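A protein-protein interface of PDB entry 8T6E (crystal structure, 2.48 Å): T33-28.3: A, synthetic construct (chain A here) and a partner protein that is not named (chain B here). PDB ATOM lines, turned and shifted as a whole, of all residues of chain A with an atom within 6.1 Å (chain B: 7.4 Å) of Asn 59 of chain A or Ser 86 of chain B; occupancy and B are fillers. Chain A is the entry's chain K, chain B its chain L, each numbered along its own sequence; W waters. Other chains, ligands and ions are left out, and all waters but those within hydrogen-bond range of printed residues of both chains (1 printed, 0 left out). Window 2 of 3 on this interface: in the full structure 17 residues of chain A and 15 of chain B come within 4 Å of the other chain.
Of the 9 printed residues of chain A, 4 touch a printed residue of chain B. Printed residues of chain A that touch a printed residue of chain B: Leu 55, Gly 58, Asn 59 and Arg 61. Hydrophobic or aromatic side chains of chain A that line the printed part of chain B: Leu 55. Along chain A the printed residues that touch a printed residue of chain B span positions 55 to 61. Printed residues of chain B that touch a printed residue of chain A: Val 80, Asp 83, Ala 84, Ser 86 and Tyr 87. Among the printed residues, 8 pairs touch across the chains.
Water W1 lies within hydrogen-bond range of OD2 of Asp 83 of chain B (2.5 Å), O of Leu 55 of chain A (2.7 Å), NZ of Lys 79 of chain B (2.9 Å) and N of Gly 58 of chain A (3.5 Å).
Among the printed residues, pairs that only touch across the chains: Asn 59 of chain A with Tyr 87 of chain B (3.4 Å), Gly 58 of chain A with Asp 83 of chain B (3.4 Å), Leu 55 of chain A with Tyr 87 of chain B (3.5 Å), Leu 55 of chain A with Val 80 of chain B (3.7 Å), Leu 55 of chain A with Ala 84 of chain B (3.7 Å) and Asn 59 of chain A with Ser 86 of chain B (3.8 Å).
Of chain B, only Asp 83, Ser 86 and Tyr 87 come within 4 Å of Asn 59 of chain A. Printed residues of chain A within 4 Å of Val 80 of chain B: Leu 55. Of the printed residues of chain A, Tyr 87 of chain B touches Leu 55 (3.5 Å), Asn 59 (3.4 Å) and Arg 61 (2.7 Å). Printed residues of chain B within 4 Å of Gly 58 of chain A: Asp 83. The nearest printed residue of chain A that does not touch Asp 83 of chain B is Leu 55 of chain A (4.1 Å).
NE2 of Gln 54 of chain A lies within hydrogen-bond range of O of Gly 58 of chain A (3.1 Å). The backbone NH (N) of Arg 61 of chain A lies close to the side-chain amide oxygen (OD1) of Asn 59 of chain A, 3.1 Å away.
The backbone NH of Asn 59 of chain A sits at hydrogen-bond distance from the side-chain carboxylate of Asp 83 of chain B, at 3.4 Å. NH1 of Arg 61 of chain A is in hydrogen-bond range of O of Tyr 87 of chain B, 2.7 Å away.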
ATOM      1  N   GLN A  54     -13.284   5.801  -3.046  1.00  0.00           N
ATOM      2  CA  GLN A  54     -13.074   5.728  -4.487  1.00  0.00           C
ATOM      3  C   GLN A  54     -11.595   5.597  -4.822  1.00  0.00           C
ATOM      4  O   GLN A  54     -11.216   4.817  -5.705  1.00  0.00           O
ATOM      5  CB  GLN A  54     -13.671   6.962  -5.165  1.00  0.00           C
ATOM      6  CG  GLN A  54     -13.330   7.086  -6.641  1.00  0.00           C
ATOM      7  CD  GLN A  54     -13.937   5.977  -7.474  1.00  0.00           C
ATOM      8  OE1 GLN A  54     -15.158   5.877  -7.599  1.00  0.00           O
ATOM      9  NE2 GLN A  54     -13.087   5.130  -8.043  1.00  0.00           N
ATOM     10  N   LEU A  55     -10.742   6.344  -4.118  1.00  0.00           N
ATOM     11  CA  LEU A  55      -9.311   6.298  -4.388  1.00  0.00           C
ATOM     12  C   LEU A  55      -8.699   4.948  -4.046  1.00  0.00           C
ATOM     13  O   LEU A  55      -7.611   4.633  -4.539  1.00  0.00           O
ATOM     14  CB  LEU A  55      -8.605   7.415  -3.622  1.00  0.00           C
ATOM     15  CG  LEU A  55      -9.118   8.801  -4.006  1.00  0.00           C
ATOM     16  CD1 LEU A  55      -8.340   9.888  -3.287  1.00  0.00           C
ATOM     17  CD2 LEU A  55      -9.050   8.984  -5.515  1.00  0.00           C
ATOM     18  N   LEU A  57     -10.292   2.151  -4.915  1.00  0.00           N
ATOM     19  CA  LEU A  57     -10.629   1.384  -6.106  1.00  0.00           C
ATOM     20  C   LEU A  57      -9.881   1.863  -7.343  1.00  0.00           C
ATOM     21  O   LEU A  57      -9.709   1.085  -8.288  1.00  0.00           O
ATOM     22  CB  LEU A  57     -12.137   1.444  -6.356  1.00  0.00           C
ATOM     23  CG  LEU A  57     -13.023   1.054  -5.169  1.00  0.00           C
ATOM     24  CD1 LEU A  57     -14.495   1.107  -5.553  1.00  0.00           C
ATOM     25  CD2 LEU A  57     -12.649  -0.323  -4.646  1.00  0.00           C
ATOM     26  N   GLY A  58      -9.440   3.106  -7.362  1.00  0.00           N
ATOM     27  CA  GLY A  58      -8.699   3.652  -8.482  1.00  0.00           C
ATOM     28  C   GLY A  58      -8.979   5.135  -8.645  1.00  0.00           C
ATOM     29  O   GLY A  58     -10.016   5.655  -8.252  1.00  0.00           O
ATOM     30  N   ASN A  59      -8.022   5.831  -9.242  1.00  0.00           N
ATOM     31  CA  ASN A  59      -8.152   7.259  -9.507  1.00  0.00           C
ATOM     32  C   ASN A  59      -9.123   7.488 -10.658  1.00  0.00           C
ATOM     33  O   ASN A  59      -8.791   7.156 -11.805  1.00  0.00           O
ATOM     34  CB  ASN A  59      -6.780   7.858  -9.822  1.00  0.00           C
ATOM     35  CG  ASN A  59      -6.836   9.351 -10.102  1.00  0.00           C
ATOM     36  OD1 ASN A  59      -7.852  10.006  -9.866  1.00  0.00           O
ATOM     37  ND2 ASN A  59      -5.737   9.895 -10.608  1.00  0.00           N
ATOM     38  N   PRO A  60     -10.315   8.045 -10.413  1.00  0.00           N
ATOM     39  CA  PRO A  60     -11.291   8.203 -11.502  1.00  0.00           C
ATOM     40  C   PRO A  60     -10.897   9.248 -12.532  1.00  0.00           C
ATOM     41  O   PRO A  60     -11.537   9.312 -13.589  1.00  0.00           O
ATOM     42  CB  PRO A  60     -12.574   8.604 -10.765  1.00  0.00           C
ATOM     43  CG  PRO A  60     -12.097   9.282  -9.530  1.00  0.00           C
ATOM     44  CD  PRO A  60     -10.813   8.590  -9.137  1.00  0.00           C
ATOM     45  N   ARG A  61      -9.877  10.065 -12.266  1.00  0.00           N
ATOM     46  CA  ARG A  61      -9.423  11.053 -13.237  1.00  0.00           C
ATOM     47  C   ARG A  61      -8.431  10.483 -14.238  1.00  0.00           C
ATOM     48  O   ARG A  61      -8.004  11.208 -15.143  1.00  0.00           O
ATOM     49  CB  ARG A  61      -8.804  12.255 -12.519  1.00  0.00           C
ATOM     50  CG  ARG A  61      -9.823  13.151 -11.838  1.00  0.00           C
ATOM     51  CD  ARG A  61      -9.161  14.160 -10.918  1.00  0.00           C
ATOM     52  NE  ARG A  61     -10.151  14.986 -10.239  1.00  0.00           N
ATOM     53  CZ  ARG A  61      -9.894  15.757  -9.192  1.00  0.00           C
ATOM     54  NH1 ARG A  61      -8.682  15.831  -8.668  1.00  0.00           N
ATOM     55  NH2 ARG A  61     -10.881  16.466  -8.651  1.00  0.00           N
ATOM     56  N   GLU A  62      -8.052   9.219 -14.093  1.00  0.00           N
ATOM     57  CA  GLU A  62      -7.195   8.576 -15.075  1.00  0.00           C
ATOM     58  C   GLU A  62      -7.891   8.554 -16.433  1.00  0.00           C
ATOM     59  O   GLU A  62      -9.073   8.189 -16.511  1.00  0.00           O
ATOM     60  CB  GLU A  62      -6.860   7.154 -14.634  1.00  0.00           C
ATOM     61  CG  GLU A  62      -6.107   6.342 -15.675  1.00  0.00           C
ATOM     62  CD  GLU A  62      -6.156   4.853 -15.395  1.00  0.00           C
ATOM     63  OE1 GLU A  62      -7.104   4.410 -14.713  1.00  0.00           O
ATOM     64  OE2 GLU A  62      -5.248   4.126 -15.853  1.00  0.00           O
ATOM     65  N   PHE A  65     -10.431   5.587 -17.632  1.00  0.00           N
ATOM     66  CA  PHE A  65     -10.624   4.884 -16.371  1.00  0.00           C
ATOM     67  C   PHE A  65     -11.638   3.760 -16.530  1.00  0.00           C
ATOM     68  O   PHE A  65     -12.823   4.012 -16.771  1.00  0.00           O
ATOM     69  CB  PHE A  65     -11.066   5.870 -15.289  1.00  0.00           C
ATOM     70  CG  PHE A  65     -11.252   5.253 -13.934  1.00  0.00           C
ATOM     71  CD1 PHE A  65     -10.200   4.609 -13.297  1.00  0.00           C
ATOM     72  CD2 PHE A  65     -12.472   5.337 -13.286  1.00  0.00           C
ATOM     73  CE1 PHE A  65     -10.370   4.045 -12.042  1.00  0.00           C
ATOM     74  CE2 PHE A  65     -12.648   4.782 -12.031  1.00  0.00           C
ATOM     75  CZ  PHE A  65     -11.596   4.133 -11.408  1.00  0.00           C
ATOM     76  N   LEU B  20      -6.270  12.461   2.155  1.00  0.00           N
ATOM     77  CA  LEU B  20      -5.173  11.502   2.233  1.00  0.00           C
ATOM     78  C   LEU B  20      -5.226  10.713   3.534  1.00  0.00           C
ATOM     79  O   LEU B  20      -4.909   9.518   3.558  1.00  0.00           O
ATOM     80  CB  LEU B  20      -3.832  12.223   2.099  1.00  0.00           C
ATOM     81  CG  LEU B  20      -3.602  12.988   0.796  1.00  0.00           C
ATOM     82  CD1 LEU B  20      -2.239  13.660   0.803  1.00  0.00           C
ATOM     83  CD2 LEU B  20      -3.739  12.055  -0.396  1.00  0.00           C
ATOM     84  N   ALA B  59       5.888  14.295  -5.382  1.00  0.00           N
ATOM     85  CA  ALA B  59       5.590  13.808  -4.045  1.00  0.00           C
ATOM     86  C   ALA B  59       6.506  12.648  -3.683  1.00  0.00           C
ATOM     87  O   ALA B  59       6.913  11.862  -4.543  1.00  0.00           O
ATOM     88  CB  ALA B  59       4.125  13.366  -3.922  1.00  0.00           C
ATOM     89  N   LYS B  79       0.048   1.533  -5.399  1.00  0.00           N
ATOM     90  CA  LYS B  79      -1.000   1.860  -6.362  1.00  0.00           C
ATOM     91  C   LYS B  79      -2.058   2.766  -5.743  1.00  0.00           C
ATOM     92  O   LYS B  79      -2.482   3.746  -6.367  1.00  0.00           O
ATOM     93  CB  LYS B  79      -1.629   0.573  -6.905  1.00  0.00           C
ATOM     94  CG  LYS B  79      -2.395   0.738  -8.215  1.00  0.00           C
ATOM     95  CD  LYS B  79      -3.857   1.083  -7.976  1.00  0.00           C
ATOM     96  CE  LYS B  79      -4.548   0.013  -7.143  1.00  0.00           C
ATOM     97  NZ  LYS B  79      -6.001   0.298  -6.972  1.00  0.00           N
ATOM     98  N   VAL B  80      -2.490   2.465  -4.515  1.00  0.00           N
ATOM     99  CA  VAL B  80      -3.518   3.281  -3.873  1.00  0.00           C
ATOM    100  C   VAL B  80      -2.962   4.650  -3.498  1.00  0.00           C
ATOM    101  O   VAL B  80      -3.635   5.675  -3.666  1.00  0.00           O
ATOM    102  CB  VAL B  80      -4.097   2.552  -2.646  1.00  0.00           C
ATOM    103  CG1 VAL B  80      -5.251   3.347  -2.051  1.00  0.00           C
ATOM    104  CG2 VAL B  80      -4.550   1.149  -3.024  1.00  0.00           C
ATOM    105  N   VAL B  81      -1.727   4.693  -2.989  1.00  0.00           N
ATOM    106  CA  VAL B  81      -1.126   5.967  -2.608  1.00  0.00           C
ATOM    107  C   VAL B  81      -0.888   6.839  -3.835  1.00  0.00           C
ATOM    108  O   VAL B  81      -1.182   8.041  -3.824  1.00  0.00           O
ATOM    109  CB  VAL B  81       0.174   5.727  -1.815  1.00  0.00           C
ATOM    110  CG1 VAL B  81       0.976   7.012  -1.698  1.00  0.00           C
ATOM    111  CG2 VAL B  81      -0.144   5.176  -0.433  1.00  0.00           C
ATOM    112  N   THR B  82      -0.358   6.253  -4.913  1.00  0.00           N
ATOM    113  CA  THR B  82      -0.131   7.024  -6.132  1.00  0.00           C
ATOM    114  C   THR B  82      -1.444   7.550  -6.700  1.00  0.00           C
ATOM    115  O   THR B  82      -1.510   8.687  -7.182  1.00  0.00           O
ATOM    116  CB  THR B  82       0.603   6.173  -7.171  1.00  0.00           C
ATOM    117  OG1 THR B  82       1.837   5.698  -6.617  1.00  0.00           O
ATOM    118  CG2 THR B  82       0.901   6.990  -8.422  1.00  0.00           C
ATOM    119  N   ASP B  83      -2.504   6.740  -6.642  1.00  0.00           N
ATOM    120  CA  ASP B  83      -3.812   7.197  -7.101  1.00  0.00           C
ATOM    121  C   ASP B  83      -4.338   8.332  -6.230  1.00  0.00           C
ATOM    122  O   ASP B  83      -4.850   9.333  -6.747  1.00  0.00           O
ATOM    123  CB  ASP B  83      -4.802   6.032  -7.115  1.00  0.00           C
ATOM    124  CG  ASP B  83      -4.580   5.091  -8.283  1.00  0.00           C
ATOM    125  OD1 ASP B  83      -3.704   5.385  -9.124  1.00  0.00           O
ATOM    126  OD2 ASP B  83      -5.284   4.062  -8.362  1.00  0.00           O
ATOM    127  N   ALA B  84      -4.216   8.195  -4.909  1.00  0.00           N
ATOM    128  CA  ALA B  84      -4.725   9.221  -4.003  1.00  0.00           C
ATOM    129  C   ALA B  84      -3.940  10.519  -4.140  1.00  0.00           C
ATOM    130  O   ALA B  84      -4.526  11.605  -4.224  1.00  0.00           O
ATOM    131  CB  ALA B  84      -4.682   8.716  -2.563  1.00  0.00           C
ATOM    132  N   ILE B  85      -2.607  10.429  -4.152  1.00  0.00           N
ATOM    133  CA  ILE B  85      -1.781  11.626  -4.284  1.00  0.00           C
ATOM    134  C   ILE B  85      -2.073  12.333  -5.602  1.00  0.00           C
ATOM    135  O   ILE B  85      -2.148  13.567  -5.660  1.00  0.00           O
ATOM    136  CB  ILE B  85      -0.289  11.262  -4.153  1.00  0.00           C
ATOM    137  CG1 ILE B  85       0.036  10.813  -2.727  1.00  0.00           C
ATOM    138  CG2 ILE B  85       0.589  12.437  -4.552  1.00  0.00           C
ATOM    139  CD1 ILE B  85       0.046  11.936  -1.716  1.00  0.00           C
ATOM    140  N   SER B  86      -2.255  11.562  -6.677  1.00  0.00           N
ATOM    141  CA  SER B  86      -2.550  12.159  -7.977  1.00  0.00           C
ATOM    142  C   SER B  86      -3.906  12.855  -7.970  1.00  0.00           C
ATOM    143  O   SER B  86      -4.043  13.968  -8.491  1.00  0.00           O
ATOM    144  CB  SER B  86      -2.502  11.092  -9.070  1.00  0.00           C
ATOM    145  OG  SER B  86      -1.468  11.366 -10.002  1.00  0.00           O
ATOM    146  N   TYR B  87      -4.918  12.217  -7.379  1.00  0.00           N
ATOM    147  CA  TYR B  87      -6.252  12.807  -7.348  1.00  0.00           C
ATOM    148  C   TYR B  87      -6.295  14.044  -6.460  1.00  0.00           C
ATOM    149  O   TYR B  87      -6.887  15.063  -6.833  1.00  0.00           O
ATOM    150  CB  TYR B  87      -7.264  11.766  -6.868  1.00  0.00           C
ATOM    151  CG  TYR B  87      -8.689  12.266  -6.796  1.00  0.00           C
ATOM    152  CD1 TYR B  87      -9.499  12.271  -7.923  1.00  0.00           C
ATOM    153  CD2 TYR B  87      -9.228  12.723  -5.599  1.00  0.00           C
ATOM    154  CE1 TYR B  87     -10.803  12.724  -7.866  1.00  0.00           C
ATOM    155  CE2 TYR B  87     -10.533  13.179  -5.532  1.00  0.00           C
ATOM    156  CZ  TYR B  87     -11.315  13.177  -6.669  1.00  0.00           C
ATOM    157  OH  TYR B  87     -12.615  13.628  -6.610  1.00  0.00           O
ATOM    158  N   VAL B  88      -5.674  13.972  -5.287  1.00  0.00           N
ATOM    159  CA  VAL B  88      -5.781  15.052  -4.312  1.00  0.00           C
ATOM    160  C   VAL B  88      -4.900  16.232  -4.703  1.00  0.00           C
ATOM    161  O   VAL B  88      -5.335  17.389  -4.664  1.00  0.00           O
ATOM    162  CB  VAL B  88      -5.434  14.531  -2.904  1.00  0.00           C
ATOM    163  CG1 VAL B  88      -5.415  15.667  -1.905  1.00  0.00           C
ATOM    164  CG2 VAL B  88      -6.427  13.466  -2.481  1.00  0.00           C
ATOM    165  N   CYS B  89      -3.653  15.962  -5.087  1.00  0.00           N
ATOM    166  CA  CYS B  89      -2.671  17.014  -5.312  1.00  0.00           C
ATOM    167  C   CYS B  89      -2.468  17.361  -6.781  1.00  0.00           C
ATOM    168  O   CYS B  89      -1.810  18.366  -7.076  1.00  0.00           O
ATOM    169  CB  CYS B  89      -1.323  16.615  -4.699  1.00  0.00           C
ATOM    170  SG  CYS B  89      -1.394  16.224  -2.936  1.00  0.00           S
ATOM    171  N   GLY B  90      -3.008  16.569  -7.704  1.00  0.00           N
ATOM    172  CA  GLY B  90      -2.761  16.816  -9.110  1.00  0.00           C
ATOM    173  C   GLY B  90      -1.361  16.485  -9.567  1.00  0.00           C
ATOM    174  O   GLY B  90      -0.948  16.931 -10.639  1.00  0.00           O
ATOM    175  N   ILE B  91      -0.616  15.714  -8.783  1.00  0.00           N
ATOM    176  CA  ILE B  91       0.745  15.322  -9.130  1.00  0.00           C
ATOM    177  C   ILE B  91       0.689  14.087 -10.019  1.00  0.00           C
ATOM    178  O   ILE B  91      -0.022  13.121  -9.718  1.00  0.00           O
ATOM    179  CB  ILE B  91       1.575  15.061  -7.863  1.00  0.00           C
ATOM    180  CG1 ILE B  91       1.618  16.318  -6.992  1.00  0.00           C
ATOM    181  CG2 ILE B  91       2.982  14.601  -8.223  1.00  0.00           C
ATOM    182  CD1 ILE B  91       2.310  16.116  -5.661  1.00  0.00           C
ATOM    183  N   VAL B  92       1.442  14.115 -11.121  1.00  0.00           N
ATOM    184  CA  VAL B  92       1.412  12.998 -12.057  1.00  0.00           C
ATOM    185  C   VAL B  92       2.073  11.769 -11.437  1.00  0.00           C
ATOM    186  O   VAL B  92       2.879  11.857 -10.502  1.00  0.00           O
ATOM    187  CB  VAL B  92       2.081  13.385 -13.386  1.00  0.00           C
ATOM    188  CG1 VAL B  92       1.214  14.381 -14.138  1.00  0.00           C
ATOM    189  CG2 VAL B  92       3.452  13.974 -13.127  1.00  0.00           C
ATOM    190  N   ALA B  93       1.722  10.600 -11.979  1.00  0.00           N
ATOM    191  CA  ALA B  93       2.138   9.338 -11.374  1.00  0.00           C
ATOM    192  C   ALA B  93       3.648   9.144 -11.443  1.00  0.00           C
ATOM    193  O   ALA B  93       4.256   8.654 -10.484  1.00  0.00           O
ATOM    194  CB  ALA B  93       1.417   8.172 -12.050  1.00  0.00           C
ATOM    195  N   ASP B  94       4.273   9.515 -12.559  1.00  0.00           N
ATOM    196  CA  ASP B  94       5.713   9.335 -12.709  1.00  0.00           C
ATOM    197  C   ASP B  94       6.526  10.365 -11.929  1.00  0.00           C
ATOM    198  O   ASP B  94       7.730  10.496 -12.174  1.00  0.00           O
ATOM    199  CB  ASP B  94       6.105   9.368 -14.192  1.00  0.00           C
ATOM    200  CG  ASP B  94       5.816  10.703 -14.849  1.00  0.00           C
ATOM    201  OD1 ASP B  94       5.085  11.521 -14.256  1.00  0.00           O
ATOM    202  OD2 ASP B  94       6.326  10.937 -15.966  1.00  0.00           O
ATOM    203  N   ILE B  96       5.882  10.504  -8.319  1.00  0.00           N
ATOM    204  CA  ILE B  96       5.467  10.116  -6.977  1.00  0.00           C
ATOM    205  C   ILE B  96       6.328   8.941  -6.537  1.00  0.00           C
ATOM    206  O   ILE B  96       6.251   7.856  -7.126  1.00  0.00           O
ATOM    207  CB  ILE B  96       3.977   9.742  -6.917  1.00  0.00           C
ATOM    208  CG1 ILE B  96       3.106  10.939  -7.303  1.00  0.00           C
ATOM    209  CG2 ILE B  96       3.613   9.225  -5.531  1.00  0.00           C
ATOM    210  CD1 ILE B  96       1.667  10.574  -7.603  1.00  0.00           C
HETATM  211  O   HOH W   1      -6.169   3.088  -6.256  1.00  0.00           O
